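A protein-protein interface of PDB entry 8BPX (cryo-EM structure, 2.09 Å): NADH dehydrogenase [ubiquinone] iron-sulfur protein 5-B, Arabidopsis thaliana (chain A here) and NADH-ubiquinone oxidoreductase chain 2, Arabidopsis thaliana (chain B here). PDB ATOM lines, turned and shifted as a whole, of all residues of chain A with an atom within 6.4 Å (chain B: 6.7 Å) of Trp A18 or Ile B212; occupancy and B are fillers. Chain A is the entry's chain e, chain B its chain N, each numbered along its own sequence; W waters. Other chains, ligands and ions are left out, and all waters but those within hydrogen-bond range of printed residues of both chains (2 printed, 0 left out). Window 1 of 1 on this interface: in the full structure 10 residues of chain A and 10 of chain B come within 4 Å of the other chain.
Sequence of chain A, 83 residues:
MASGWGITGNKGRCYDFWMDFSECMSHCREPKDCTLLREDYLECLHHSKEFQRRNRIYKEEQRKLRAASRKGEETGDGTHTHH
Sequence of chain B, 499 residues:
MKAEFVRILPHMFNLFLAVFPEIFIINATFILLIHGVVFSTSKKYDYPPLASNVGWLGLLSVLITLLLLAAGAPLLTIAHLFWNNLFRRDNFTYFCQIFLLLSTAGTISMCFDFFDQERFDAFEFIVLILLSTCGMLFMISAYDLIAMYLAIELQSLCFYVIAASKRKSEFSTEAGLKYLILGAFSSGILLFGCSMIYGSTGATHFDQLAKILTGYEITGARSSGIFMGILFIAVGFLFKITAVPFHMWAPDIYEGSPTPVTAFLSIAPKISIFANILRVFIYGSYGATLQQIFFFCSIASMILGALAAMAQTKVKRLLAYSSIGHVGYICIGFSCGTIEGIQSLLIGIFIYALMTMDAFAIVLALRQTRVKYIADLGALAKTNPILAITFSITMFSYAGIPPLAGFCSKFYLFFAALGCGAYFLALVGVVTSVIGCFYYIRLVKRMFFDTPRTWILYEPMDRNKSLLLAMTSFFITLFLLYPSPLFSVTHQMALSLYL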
ATOM      1  N   ALA A   2      -4.588  -4.208 -30.827  1.00  0.00           N
ATOM      2  CA  ALA A   2      -4.943  -4.994 -29.631  1.00  0.00           C
ATOM      3  C   ALA A   2      -4.099  -6.227 -29.310  1.00  0.00           C
ATOM      4  O   ALA A   2      -4.181  -6.634 -28.238  1.00  0.00           O
ATOM      5  CB  ALA A   2      -6.415  -5.312 -29.744  1.00  0.00           C
ATOM      6  N   SER A   3      -3.475  -6.838 -30.321  1.00  0.00           N
ATOM      7  CA  SER A   3      -2.761  -8.127 -30.125  1.00  0.00           C
ATOM      8  C   SER A   3      -1.528  -7.964 -29.238  1.00  0.00           C
ATOM      9  O   SER A   3      -1.159  -8.928 -28.616  1.00  0.00           O
ATOM     10  CB  SER A   3      -2.381  -8.765 -31.497  1.00  0.00           C
ATOM     11  OG  SER A   3      -1.196  -8.202 -32.025  1.00  0.00           O
ATOM     12  N   CYS A  14       0.224   0.832 -29.326  1.00  0.00           N
ATOM     13  CA  CYS A  14      -1.088   1.089 -28.695  1.00  0.00           C
ATOM     14  C   CYS A  14      -1.596  -0.026 -27.746  1.00  0.00           C
ATOM     15  O   CYS A  14      -2.661   0.092 -27.281  1.00  0.00           O
ATOM     16  CB  CYS A  14      -2.090   1.332 -29.813  1.00  0.00           C
ATOM     17  SG  CYS A  14      -1.601   2.683 -30.907  1.00  0.00           S
ATOM     18  N   TYR A  15      -0.790  -1.000 -27.443  1.00  0.00           N
ATOM     19  CA  TYR A  15      -1.156  -2.155 -26.598  1.00  0.00           C
ATOM     20  C   TYR A  15      -1.394  -1.795 -25.110  1.00  0.00           C
ATOM     21  O   TYR A  15      -2.336  -2.300 -24.612  1.00  0.00           O
ATOM     22  CB  TYR A  15      -0.111  -3.253 -26.754  1.00  0.00           C
ATOM     23  CG  TYR A  15      -0.449  -4.463 -25.940  1.00  0.00           C
ATOM     24  CD1 TYR A  15      -1.511  -5.270 -26.305  1.00  0.00           C
ATOM     25  CD2 TYR A  15       0.248  -4.756 -24.785  1.00  0.00           C
ATOM     26  CE1 TYR A  15      -1.835  -6.393 -25.571  1.00  0.00           C
ATOM     27  CE2 TYR A  15      -0.057  -5.876 -24.038  1.00  0.00           C
ATOM     28  CZ  TYR A  15      -1.097  -6.692 -24.443  1.00  0.00           C
ATOM     29  OH  TYR A  15      -1.428  -7.768 -23.705  1.00  0.00           O
ATOM     30  N   ASP A  16      -0.635  -0.894 -24.512  1.00  0.00           N
ATOM     31  CA  ASP A  16      -0.917  -0.519 -23.132  1.00  0.00           C
ATOM     32  C   ASP A  16      -2.249   0.216 -23.021  1.00  0.00           C
ATOM     33  O   ASP A  16      -3.017  -0.024 -22.082  1.00  0.00           O
ATOM     34  CB  ASP A  16       0.238   0.314 -22.584  1.00  0.00           C
ATOM     35  CG  ASP A  16       1.454  -0.537 -22.265  1.00  0.00           C
ATOM     36  OD1 ASP A  16       1.288  -1.761 -22.103  1.00  0.00           O
ATOM     37  OD2 ASP A  16       2.573   0.007 -22.193  1.00  0.00           O
ATOM     38  N   PHE A  17      -2.555   1.088 -23.985  1.00  0.00           N
ATOM     39  CA  PHE A  17      -3.866   1.731 -24.015  1.00  0.00           C
ATOM     40  C   PHE A  17      -4.977   0.701 -24.157  1.00  0.00           C
ATOM     41  O   PHE A  17      -6.005   0.778 -23.470  1.00  0.00           O
ATOM     42  CB  PHE A  17      -3.939   2.733 -25.168  1.00  0.00           C
ATOM     43  CG  PHE A  17      -3.183   4.004 -24.927  1.00  0.00           C
ATOM     44  CD1 PHE A  17      -3.612   4.917 -23.979  1.00  0.00           C
ATOM     45  CD2 PHE A  17      -2.053   4.300 -25.670  1.00  0.00           C
ATOM     46  CE1 PHE A  17      -2.914   6.092 -23.765  1.00  0.00           C
ATOM     47  CE2 PHE A  17      -1.353   5.474 -25.461  1.00  0.00           C
ATOM     48  CZ  PHE A  17      -1.782   6.368 -24.509  1.00  0.00           C
ATOM     49  N   TRP A  18      -4.775  -0.248 -25.075  1.00  0.00           N
ATOM     50  CA  TRP A  18      -5.744  -1.338 -25.242  1.00  0.00           C
ATOM     51  C   TRP A  18      -5.981  -2.068 -23.905  1.00  0.00           C
ATOM     52  O   TRP A  18      -7.095  -2.363 -23.638  1.00  0.00           O
ATOM     53  CB  TRP A  18      -5.327  -2.323 -26.351  1.00  0.00           C
ATOM     54  CG  TRP A  18      -6.237  -3.508 -26.349  1.00  0.00           C
ATOM     55  CD1 TRP A  18      -5.977  -4.766 -25.895  1.00  0.00           C
ATOM     56  CD2 TRP A  18      -7.616  -3.494 -26.724  1.00  0.00           C
ATOM     57  NE1 TRP A  18      -7.095  -5.542 -25.995  1.00  0.00           N
ATOM     58  CE2 TRP A  18      -8.117  -4.794 -26.506  1.00  0.00           C
ATOM     59  CE3 TRP A  18      -8.468  -2.514 -27.235  1.00  0.00           C
ATOM     60  CZ2 TRP A  18      -9.437  -5.128 -26.780  1.00  0.00           C
ATOM     61  CZ3 TRP A  18      -9.767  -2.852 -27.505  1.00  0.00           C
ATOM     62  CH2 TRP A  18     -10.246  -4.143 -27.288  1.00  0.00           C
ATOM     63  N   MET A  19      -4.925  -2.413 -23.224  1.00  0.00           N
ATOM     64  CA  MET A  19      -5.056  -3.213 -22.014  1.00  0.00           C
ATOM     65  C   MET A  19      -5.716  -2.417 -20.896  1.00  0.00           C
ATOM     66  O   MET A  19      -6.511  -2.969 -20.130  1.00  0.00           O
ATOM     67  CB  MET A  19      -3.690  -3.743 -21.583  1.00  0.00           C
ATOM     68  CG  MET A  19      -3.130  -4.798 -22.521  1.00  0.00           C
ATOM     69  SD  MET A  19      -4.281  -6.140 -22.892  1.00  0.00           S
ATOM     70  CE  MET A  19      -4.204  -7.066 -21.369  1.00  0.00           C
ATOM     71  N   ASP A  20      -5.418  -1.118 -20.791  1.00  0.00           N
ATOM     72  CA  ASP A  20      -6.140  -0.282 -19.833  1.00  0.00           C
ATOM     73  C   ASP A  20      -7.629  -0.256 -20.145  1.00  0.00           C
ATOM     74  O   ASP A  20      -8.468  -0.409 -19.249  1.00  0.00           O
ATOM     75  CB  ASP A  20      -5.581   1.144 -19.814  1.00  0.00           C
ATOM     76  CG  ASP A  20      -4.083   1.187 -19.660  1.00  0.00           C
ATOM     77  OD1 ASP A  20      -3.542   0.370 -18.889  1.00  0.00           O
ATOM     78  OD2 ASP A  20      -3.443   2.049 -20.300  1.00  0.00           O
ATOM     79  N   PHE A  21      -7.980  -0.081 -21.422  1.00  0.00           N
ATOM     80  CA  PHE A  21      -9.390  -0.055 -21.799  1.00  0.00           C
ATOM     81  C   PHE A  21     -10.076  -1.387 -21.502  1.00  0.00           C
ATOM     82  O   PHE A  21     -11.192  -1.414 -20.968  1.00  0.00           O
ATOM     83  CB  PHE A  21      -9.521   0.302 -23.278  1.00  0.00           C
ATOM     84  CG  PHE A  21     -10.895   0.101 -23.833  1.00  0.00           C
ATOM     85  CD1 PHE A  21     -11.966   0.826 -23.347  1.00  0.00           C
ATOM     86  CD2 PHE A  21     -11.116  -0.813 -24.852  1.00  0.00           C
ATOM     87  CE1 PHE A  21     -13.232   0.642 -23.859  1.00  0.00           C
ATOM     88  CE2 PHE A  21     -12.382  -0.998 -25.371  1.00  0.00           C
ATOM     89  CZ  PHE A  21     -13.439  -0.270 -24.875  1.00  0.00           C
ATOM     90  N   SER A  22      -9.422  -2.501 -21.846  1.00  0.00           N
ATOM     91  CA  SER A  22     -10.003  -3.818 -21.608  1.00  0.00           C
ATOM     92  C   SER A  22     -10.173  -4.089 -20.119  1.00  0.00           C
ATOM     93  O   SER A  22     -11.207  -4.614 -19.691  1.00  0.00           O
ATOM     94  CB  SER A  22      -9.136  -4.903 -22.248  1.00  0.00           C
ATOM     95  OG  SER A  22      -9.005  -4.697 -23.641  1.00  0.00           O
ATOM     96  N   GLU A  23      -9.166  -3.740 -19.316  1.00  0.00           N
ATOM     97  CA  GLU A  23      -9.259  -3.950 -17.876  1.00  0.00           C
ATOM     98  C   GLU A  23     -10.363  -3.090 -17.271  1.00  0.00           C
ATOM     99  O   GLU A  23     -11.069  -3.533 -16.359  1.00  0.00           O
ATOM    100  CB  GLU A  23      -7.893  -3.676 -17.234  1.00  0.00           C
ATOM    101  CG  GLU A  23      -7.790  -3.807 -15.715  1.00  0.00           C
ATOM    102  CD  GLU A  23      -8.503  -2.706 -14.955  1.00  0.00           C
ATOM    103  OE1 GLU A  23      -9.359  -3.026 -14.109  1.00  0.00           O
ATOM    104  OE2 GLU A  23      -8.217  -1.520 -15.219  1.00  0.00           O
ATOM    105  N   MET A  25     -13.173  -2.091 -18.892  1.00  0.00           N
ATOM    106  CA  MET A  25     -14.444  -2.677 -19.303  1.00  0.00           C
ATOM    107  C   MET A  25     -14.712  -4.022 -18.639  1.00  0.00           C
ATOM    108  O   MET A  25     -15.872  -4.435 -18.557  1.00  0.00           O
ATOM    109  CB  MET A  25     -14.486  -2.819 -20.827  1.00  0.00           C
ATOM    110  CG  MET A  25     -14.732  -1.496 -21.547  1.00  0.00           C
ATOM    111  SD  MET A  25     -16.428  -1.200 -22.095  1.00  0.00           S
ATOM    112  CE  MET A  25     -16.778  -2.701 -23.005  1.00  0.00           C
ATOM    113  N   LEU A  37     -10.717   6.006 -21.685  1.00  0.00           N
ATOM    114  CA  LEU A  37      -9.683   5.045 -22.060  1.00  0.00           C
ATOM    115  C   LEU A  37      -9.880   4.552 -23.491  1.00  0.00           C
ATOM    116  O   LEU A  37      -8.906   4.353 -24.231  1.00  0.00           O
ATOM    117  CB  LEU A  37      -9.677   3.877 -21.072  1.00  0.00           C
ATOM    118  CG  LEU A  37      -9.582   4.259 -19.590  1.00  0.00           C
ATOM    119  CD1 LEU A  37      -9.374   3.039 -18.710  1.00  0.00           C
ATOM    120  CD2 LEU A  37      -8.468   5.258 -19.366  1.00  0.00           C
ATOM    121  N   ARG A  38     -11.135   4.354 -23.900  1.00  0.00           N
ATOM    122  CA  ARG A  38     -11.413   3.922 -25.266  1.00  0.00           C
ATOM    123  C   ARG A  38     -10.967   4.963 -26.284  1.00  0.00           C
ATOM    124  O   ARG A  38     -10.359   4.626 -27.311  1.00  0.00           O
ATOM    125  CB  ARG A  38     -12.902   3.635 -25.423  1.00  0.00           C
ATOM    126  CG  ARG A  38     -13.292   3.090 -26.777  1.00  0.00           C
ATOM    127  CD  ARG A  38     -14.735   3.411 -27.064  1.00  0.00           C
ATOM    128  NE  ARG A  38     -15.264   2.703 -28.221  1.00  0.00           N
ATOM    129  CZ  ARG A  38     -15.577   3.286 -29.369  1.00  0.00           C
ATOM    130  NH1 ARG A  38     -15.424   4.587 -29.549  1.00  0.00           N
ATOM    131  NH2 ARG A  38     -16.057   2.544 -30.362  1.00  0.00           N
ATOM    132  N   TYR A  41      -7.172   4.866 -26.593  1.00  0.00           N
ATOM    133  CA  TYR A  41      -6.790   3.751 -27.516  1.00  0.00           C
ATOM    134  C   TYR A  41      -6.994   4.169 -28.987  1.00  0.00           C
ATOM    135  O   TYR A  41      -6.047   4.104 -29.705  1.00  0.00           O
ATOM    136  CB  TYR A  41      -7.524   2.463 -27.125  1.00  0.00           C
ATOM    137  CG  TYR A  41      -7.351   1.371 -28.157  1.00  0.00           C
ATOM    138  CD1 TYR A  41      -6.128   0.755 -28.329  1.00  0.00           C
ATOM    139  CD2 TYR A  41      -8.384   1.012 -29.007  1.00  0.00           C
ATOM    140  CE1 TYR A  41      -5.943  -0.232 -29.282  1.00  0.00           C
ATOM    141  CE2 TYR A  41      -8.224   0.029 -29.971  1.00  0.00           C
ATOM    142  CZ  TYR A  41      -6.993  -0.594 -30.107  1.00  0.00           C
ATOM    143  OH  TYR A  41      -6.793  -1.562 -31.036  1.00  0.00           O
ATOM    144  N   LEU A  42      -8.170   4.685 -29.327  1.00  0.00           N
ATOM    145  CA  LEU A  42      -8.421   5.033 -30.724  1.00  0.00           C
ATOM    146  C   LEU A  42      -7.560   6.210 -31.183  1.00  0.00           C
ATOM    147  O   LEU A  42      -7.147   6.255 -32.351  1.00  0.00           O
ATOM    148  CB  LEU A  42      -9.907   5.320 -30.933  1.00  0.00           C
ATOM    149  CG  LEU A  42     -10.834   4.121 -30.690  1.00  0.00           C
ATOM    150  CD1 LEU A  42     -12.287   4.499 -30.918  1.00  0.00           C
ATOM    151  CD2 LEU A  42     -10.451   2.928 -31.559  1.00  0.00           C
ATOM    152  N   SER B 200      -9.824  -0.017 -38.813  1.00  0.00           N
ATOM    153  CA  SER B 200     -10.504   0.959 -37.968  1.00  0.00           C
ATOM    154  C   SER B 200     -10.342   0.658 -36.480  1.00  0.00           C
ATOM    155  O   SER B 200     -10.317   1.582 -35.661  1.00  0.00           O
ATOM    156  CB  SER B 200     -11.983   1.024 -38.335  1.00  0.00           C
ATOM    157  OG  SER B 200     -12.164   1.465 -39.665  1.00  0.00           O
ATOM    158  N   THR B 201     -10.246  -0.618 -36.099  1.00  0.00           N
ATOM    159  CA  THR B 201     -10.213  -0.979 -34.687  1.00  0.00           C
ATOM    160  C   THR B 201      -8.891  -1.563 -34.212  1.00  0.00           C
ATOM    161  O   THR B 201      -8.674  -1.636 -32.999  1.00  0.00           O
ATOM    162  CB  THR B 201     -11.329  -1.983 -34.359  1.00  0.00           C
ATOM    163  OG1 THR B 201     -10.967  -3.282 -34.849  1.00  0.00           O
ATOM    164  CG2 THR B 201     -12.642  -1.552 -34.977  1.00  0.00           C
ATOM    165  N   GLY B 202      -7.948  -1.900 -35.037  1.00  0.00           N
ATOM    166  CA  GLY B 202      -6.783  -2.637 -34.576  1.00  0.00           C
ATOM    167  C   GLY B 202      -7.065  -4.044 -34.035  1.00  0.00           C
ATOM    168  O   GLY B 202      -6.168  -4.598 -33.428  1.00  0.00           O
ATOM    169  N   ALA B 203      -8.224  -4.638 -34.317  1.00  0.00           N
ATOM    170  CA  ALA B 203      -8.548  -5.932 -33.737  1.00  0.00           C
ATOM    171  C   ALA B 203      -9.243  -6.819 -34.762  1.00  0.00           C
ATOM    172  O   ALA B 203      -9.943  -6.336 -35.654  1.00  0.00           O
ATOM    173  CB  ALA B 203      -9.437  -5.778 -32.500  1.00  0.00           C
ATOM    174  N   ASP B 207     -13.865 -11.057 -29.230  1.00  0.00           N
ATOM    175  CA  ASP B 207     -13.971 -10.415 -27.920  1.00  0.00           C
ATOM    176  C   ASP B 207     -13.538  -8.956 -27.987  1.00  0.00           C
ATOM    177  O   ASP B 207     -14.220  -8.062 -27.464  1.00  0.00           O
ATOM    178  CB  ASP B 207     -13.118 -11.164 -26.898  1.00  0.00           C
ATOM    179  CG  ASP B 207     -13.878 -12.257 -26.194  1.00  0.00           C
ATOM    180  OD1 ASP B 207     -13.224 -13.127 -25.587  1.00  0.00           O
ATOM    181  OD2 ASP B 207     -15.123 -12.254 -26.253  1.00  0.00           O
ATOM    182  N   GLN B 208     -12.393  -8.700 -28.626  1.00  0.00           N
ATOM    183  CA  GLN B 208     -11.901  -7.336 -28.763  1.00  0.00           C
ATOM    184  C   GLN B 208     -12.885  -6.478 -29.546  1.00  0.00           C
ATOM    185  O   GLN B 208     -13.157  -5.333 -29.172  1.00  0.00           O
ATOM    186  CB  GLN B 208     -10.534  -7.342 -29.446  1.00  0.00           C
ATOM    187  CG  GLN B 208      -9.489  -8.220 -28.772  1.00  0.00           C
ATOM    188  CD  GLN B 208      -8.272  -8.469 -29.649  1.00  0.00           C
ATOM    189  OE1 GLN B 208      -8.348  -8.392 -30.875  1.00  0.00           O
ATOM    190  NE2 GLN B 208      -7.142  -8.767 -29.021  1.00  0.00           N
ATOM    191  N   LEU B 209     -13.431  -7.024 -30.634  1.00  0.00           N
ATOM    192  CA  LEU B 209     -14.419  -6.294 -31.419  1.00  0.00           C
ATOM    193  C   LEU B 209     -15.655  -5.981 -30.589  1.00  0.00           C
ATOM    194  O   LEU B 209     -16.207  -4.879 -30.677  1.00  0.00           O
ATOM    195  CB  LEU B 209     -14.795  -7.098 -32.662  1.00  0.00           C
ATOM    196  CG  LEU B 209     -13.669  -7.265 -33.686  1.00  0.00           C
ATOM    197  CD1 LEU B 209     -14.122  -8.114 -34.872  1.00  0.00           C
ATOM    198  CD2 LEU B 209     -13.170  -5.906 -34.141  1.00  0.00           C
ATOM    199  N   ALA B 210     -16.098  -6.936 -29.770  1.00  0.00           N
ATOM    200  CA  ALA B 210     -17.239  -6.686 -28.899  1.00  0.00           C
ATOM    201  C   ALA B 210     -16.948  -5.537 -27.940  1.00  0.00           C
ATOM    202  O   ALA B 210     -17.764  -4.624 -27.786  1.00  0.00           O
ATOM    203  CB  ALA B 210     -17.606  -7.959 -28.132  1.00  0.00           C
ATOM    204  N   LYS B 211     -15.771  -5.548 -27.309  1.00  0.00           N
ATOM    205  CA  LYS B 211     -15.449  -4.485 -26.358  1.00  0.00           C
ATOM    206  C   LYS B 211     -15.383  -3.120 -27.037  1.00  0.00           C
ATOM    207  O   LYS B 211     -15.922  -2.137 -26.515  1.00  0.00           O
ATOM    208  CB  LYS B 211     -14.135  -4.790 -25.643  1.00  0.00           C
ATOM    209  CG  LYS B 211     -14.280  -5.736 -24.468  1.00  0.00           C
ATOM    210  CD  LYS B 211     -12.933  -6.263 -24.014  1.00  0.00           C
ATOM    211  CE  LYS B 211     -13.028  -6.928 -22.654  1.00  0.00           C
ATOM    212  NZ  LYS B 211     -13.885  -8.139 -22.696  1.00  0.00           N
ATOM    213  N   ILE B 212     -14.736  -3.036 -28.202  1.00  0.00           N
ATOM    214  CA  ILE B 212     -14.572  -1.746 -28.871  1.00  0.00           C
ATOM    215  C   ILE B 212     -15.922  -1.197 -29.313  1.00  0.00           C
ATOM    216  O   ILE B 212     -16.226  -0.015 -29.115  1.00  0.00           O
ATOM    217  CB  ILE B 212     -13.607  -1.867 -30.065  1.00  0.00           C
ATOM    218  CG1 ILE B 212     -12.165  -1.997 -29.593  1.00  0.00           C
ATOM    219  CG2 ILE B 212     -13.723  -0.650 -30.966  1.00  0.00           C
ATOM    220  CD1 ILE B 212     -11.308  -2.852 -30.496  1.00  0.00           C
ATOM    221  N   LEU B 213     -16.695  -2.018 -30.000  1.00  0.00           N
ATOM    222  CA  LEU B 213     -17.976  -1.563 -30.614  1.00  0.00           C
ATOM    223  C   LEU B 213     -19.136  -1.386 -29.626  1.00  0.00           C
ATOM    224  O   LEU B 213     -20.008  -0.648 -29.981  1.00  0.00           O
ATOM    225  CB  LEU B 213     -18.354  -2.529 -31.742  1.00  0.00           C
ATOM    226  CG  LEU B 213     -17.365  -2.774 -32.878  1.00  0.00           C
ATOM    227  CD1 LEU B 213     -18.096  -3.345 -34.073  1.00  0.00           C
ATOM    228  CD2 LEU B 213     -16.628  -1.510 -33.279  1.00  0.00           C
ATOM    229  N   THR B 214     -19.108  -1.944 -28.423  1.00  0.00           N
ATOM    230  CA  THR B 214     -20.265  -1.876 -27.539  1.00  0.00           C
ATOM    231  C   THR B 214     -20.372  -0.508 -26.881  1.00  0.00           C
ATOM    232  O   THR B 214     -19.366   0.096 -26.499  1.00  0.00           O
ATOM    233  CB  THR B 214     -20.204  -2.955 -26.458  1.00  0.00           C
ATOM    234  OG1 THR B 214     -18.857  -3.111 -25.998  1.00  0.00           O
ATOM    235  CG2 THR B 214     -20.723  -4.280 -26.998  1.00  0.00           C
ATOM    236  N   GLY B 215     -21.607  -0.028 -26.747  1.00  0.00           N
ATOM    237  CA  GLY B 215     -21.885   1.242 -26.120  1.00  0.00           C
ATOM    238  C   GLY B 215     -21.881   2.437 -27.043  1.00  0.00           C
ATOM    239  O   GLY B 215     -22.128   3.557 -26.577  1.00  0.00           O
ATOM    240  N   TYR B 216     -21.599   2.253 -28.324  1.00  0.00           N
ATOM    241  CA  TYR B 216     -21.511   3.417 -29.197  1.00  0.00           C
ATOM    242  C   TYR B 216     -22.361   3.312 -30.449  1.00  0.00           C
ATOM    243  O   TYR B 216     -22.992   4.303 -30.825  1.00  0.00           O
ATOM    244  CB  TYR B 216     -20.044   3.670 -29.574  1.00  0.00           C
ATOM    245  CG  TYR B 216     -19.221   4.068 -28.382  1.00  0.00           C
ATOM    246  CD1 TYR B 216     -18.693   3.113 -27.528  1.00  0.00           C
ATOM    247  CD2 TYR B 216     -18.991   5.404 -28.095  1.00  0.00           C
ATOM    248  CE1 TYR B 216     -17.964   3.474 -26.425  1.00  0.00           C
ATOM    249  CE2 TYR B 216     -18.248   5.777 -26.995  1.00  0.00           C
ATOM    250  CZ  TYR B 216     -17.735   4.807 -26.165  1.00  0.00           C
ATOM    251  OH  TYR B 216     -16.993   5.166 -25.065  1.00  0.00           O
ATOM    252  N   ILE B 226     -15.603   1.150 -39.748  1.00  0.00           N
ATOM    253  CA  ILE B 226     -16.363   0.091 -39.035  1.00  0.00           C
ATOM    254  C   ILE B 226     -17.725  -0.139 -39.700  1.00  0.00           C
ATOM    255  O   ILE B 226     -18.029  -1.303 -39.964  1.00  0.00           O
ATOM    256  CB  ILE B 226     -16.523   0.422 -37.548  1.00  0.00           C
ATOM    257  CG1 ILE B 226     -15.180   0.516 -36.827  1.00  0.00           C
ATOM    258  CG2 ILE B 226     -17.438  -0.585 -36.864  1.00  0.00           C
ATOM    259  CD1 ILE B 226     -15.299   1.018 -35.409  1.00  0.00           C
ATOM    260  N   SER B 285     -21.268  -5.608 -32.296  1.00  0.00           N
ATOM    261  CA  SER B 285     -22.111  -4.406 -32.083  1.00  0.00           C
ATOM    262  C   SER B 285     -22.045  -3.279 -33.081  1.00  0.00           C
ATOM    263  O   SER B 285     -21.219  -2.413 -32.865  1.00  0.00           O
ATOM    264  CB  SER B 285     -21.864  -3.827 -30.745  1.00  0.00           C
ATOM    265  OG  SER B 285     -22.667  -4.469 -29.761  1.00  0.00           O
HETATM  266  O   HOH W   1     -16.601   2.201 -23.675  1.00  0.00           O
HETATM  267  O   HOH W   2      -4.586  -7.106 -33.413  1.00  0.00           O
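Of the 16 printed residues of chain B, 7 touch a printed residue of chain A.
Hydrophobic or aromatic side chains of chain B within 4 Å of the printed part of chain A: Ile B212 and Tyr B216.
O of Gly B202 lies within hydrogen-bond range of N of Ala A2, at 3.1 Å.
NH2 of Arg A38 is in hydrogen-bond range of O of Ile B212, at 2.9 Å.
The backbone carbonyl oxygen of Thr B201 lies within hydrogen-bond range of the side-chain hydroxyl of Tyr A41 (2.7 Å).
The side-chain hydroxyl (OG1) of Thr B201 lies within hydrogen-bond range of the backbone NH (N) of Ala B203, at 3.1 Å.
The backbone carbonyl oxygen of Trp A18 lies close to the side-chain hydroxyl of Ser A22.
The backbone carbonyl oxygen of Ala B210 is in hydrogen-bond range of the side-chain hydroxyl of Thr B214 (2.6 Å).
The backbone carbonyl oxygen of Lys B211 is in hydrogen-bond range of the side-chain hydroxyl of Thr B214, at 3.1 Å.
The side-chain hydroxyl of Tyr A41 is in hydrogen-bond range of the backbone NH of Ala A2, at 3.5 Å.
Water W2 bridges the backbone carbonyl oxygen (O) of Gly B202 (3.0 Å) and the backbone NH (N) of Ser A3 (3.3 Å).
Water W1 bridges OH of Tyr B216 (3.3 Å) and SD of Met A25 (3.8 Å).
Of the printed residues of chain B, Ala A2 touches Gly B202 and Gln B208.
Trp A18 touches two residues of chain B.
Of the printed residues of chain B, Phe A21 touches Lys B211 (3.5 Å).
Of the printed residues of chain A, Lys B211 touches Phe A21 (3.5 Å) and Met A25 (3.7 Å).
Of chain A, only Trp A18 and Arg A38 come within 4 Å of Ile B212.
Of the printed residues of chain A, Tyr B216 touches Arg A38 (3.3 Å).
The nearest residue of chain A that does not touch Ile B212 is Phe A21 (4.2 Å).
The nearest printed residue of chain B that does not touch Met A25 is Ala B210 (5.2 Å).
NE2 of Gln B208 touches CB of Ala A2 (3.6 Å).
Trp A18 touches Gln B208 (CZ2 to CB, 3.6 Å).
Trp A18 touches Ile B212.
O of Lys B211 touches CZ of Phe A21, 3.5 Å away.
CE of Met A25 touches O of Lys B211, 3.7 Å away.
OG1 of Thr B214 touches CE of Met A25, 3.7 Å away.
CE1 of Tyr B216 touches CD of Arg A38, 3.3 Å away.
Gly B202 touches Tyr A41.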
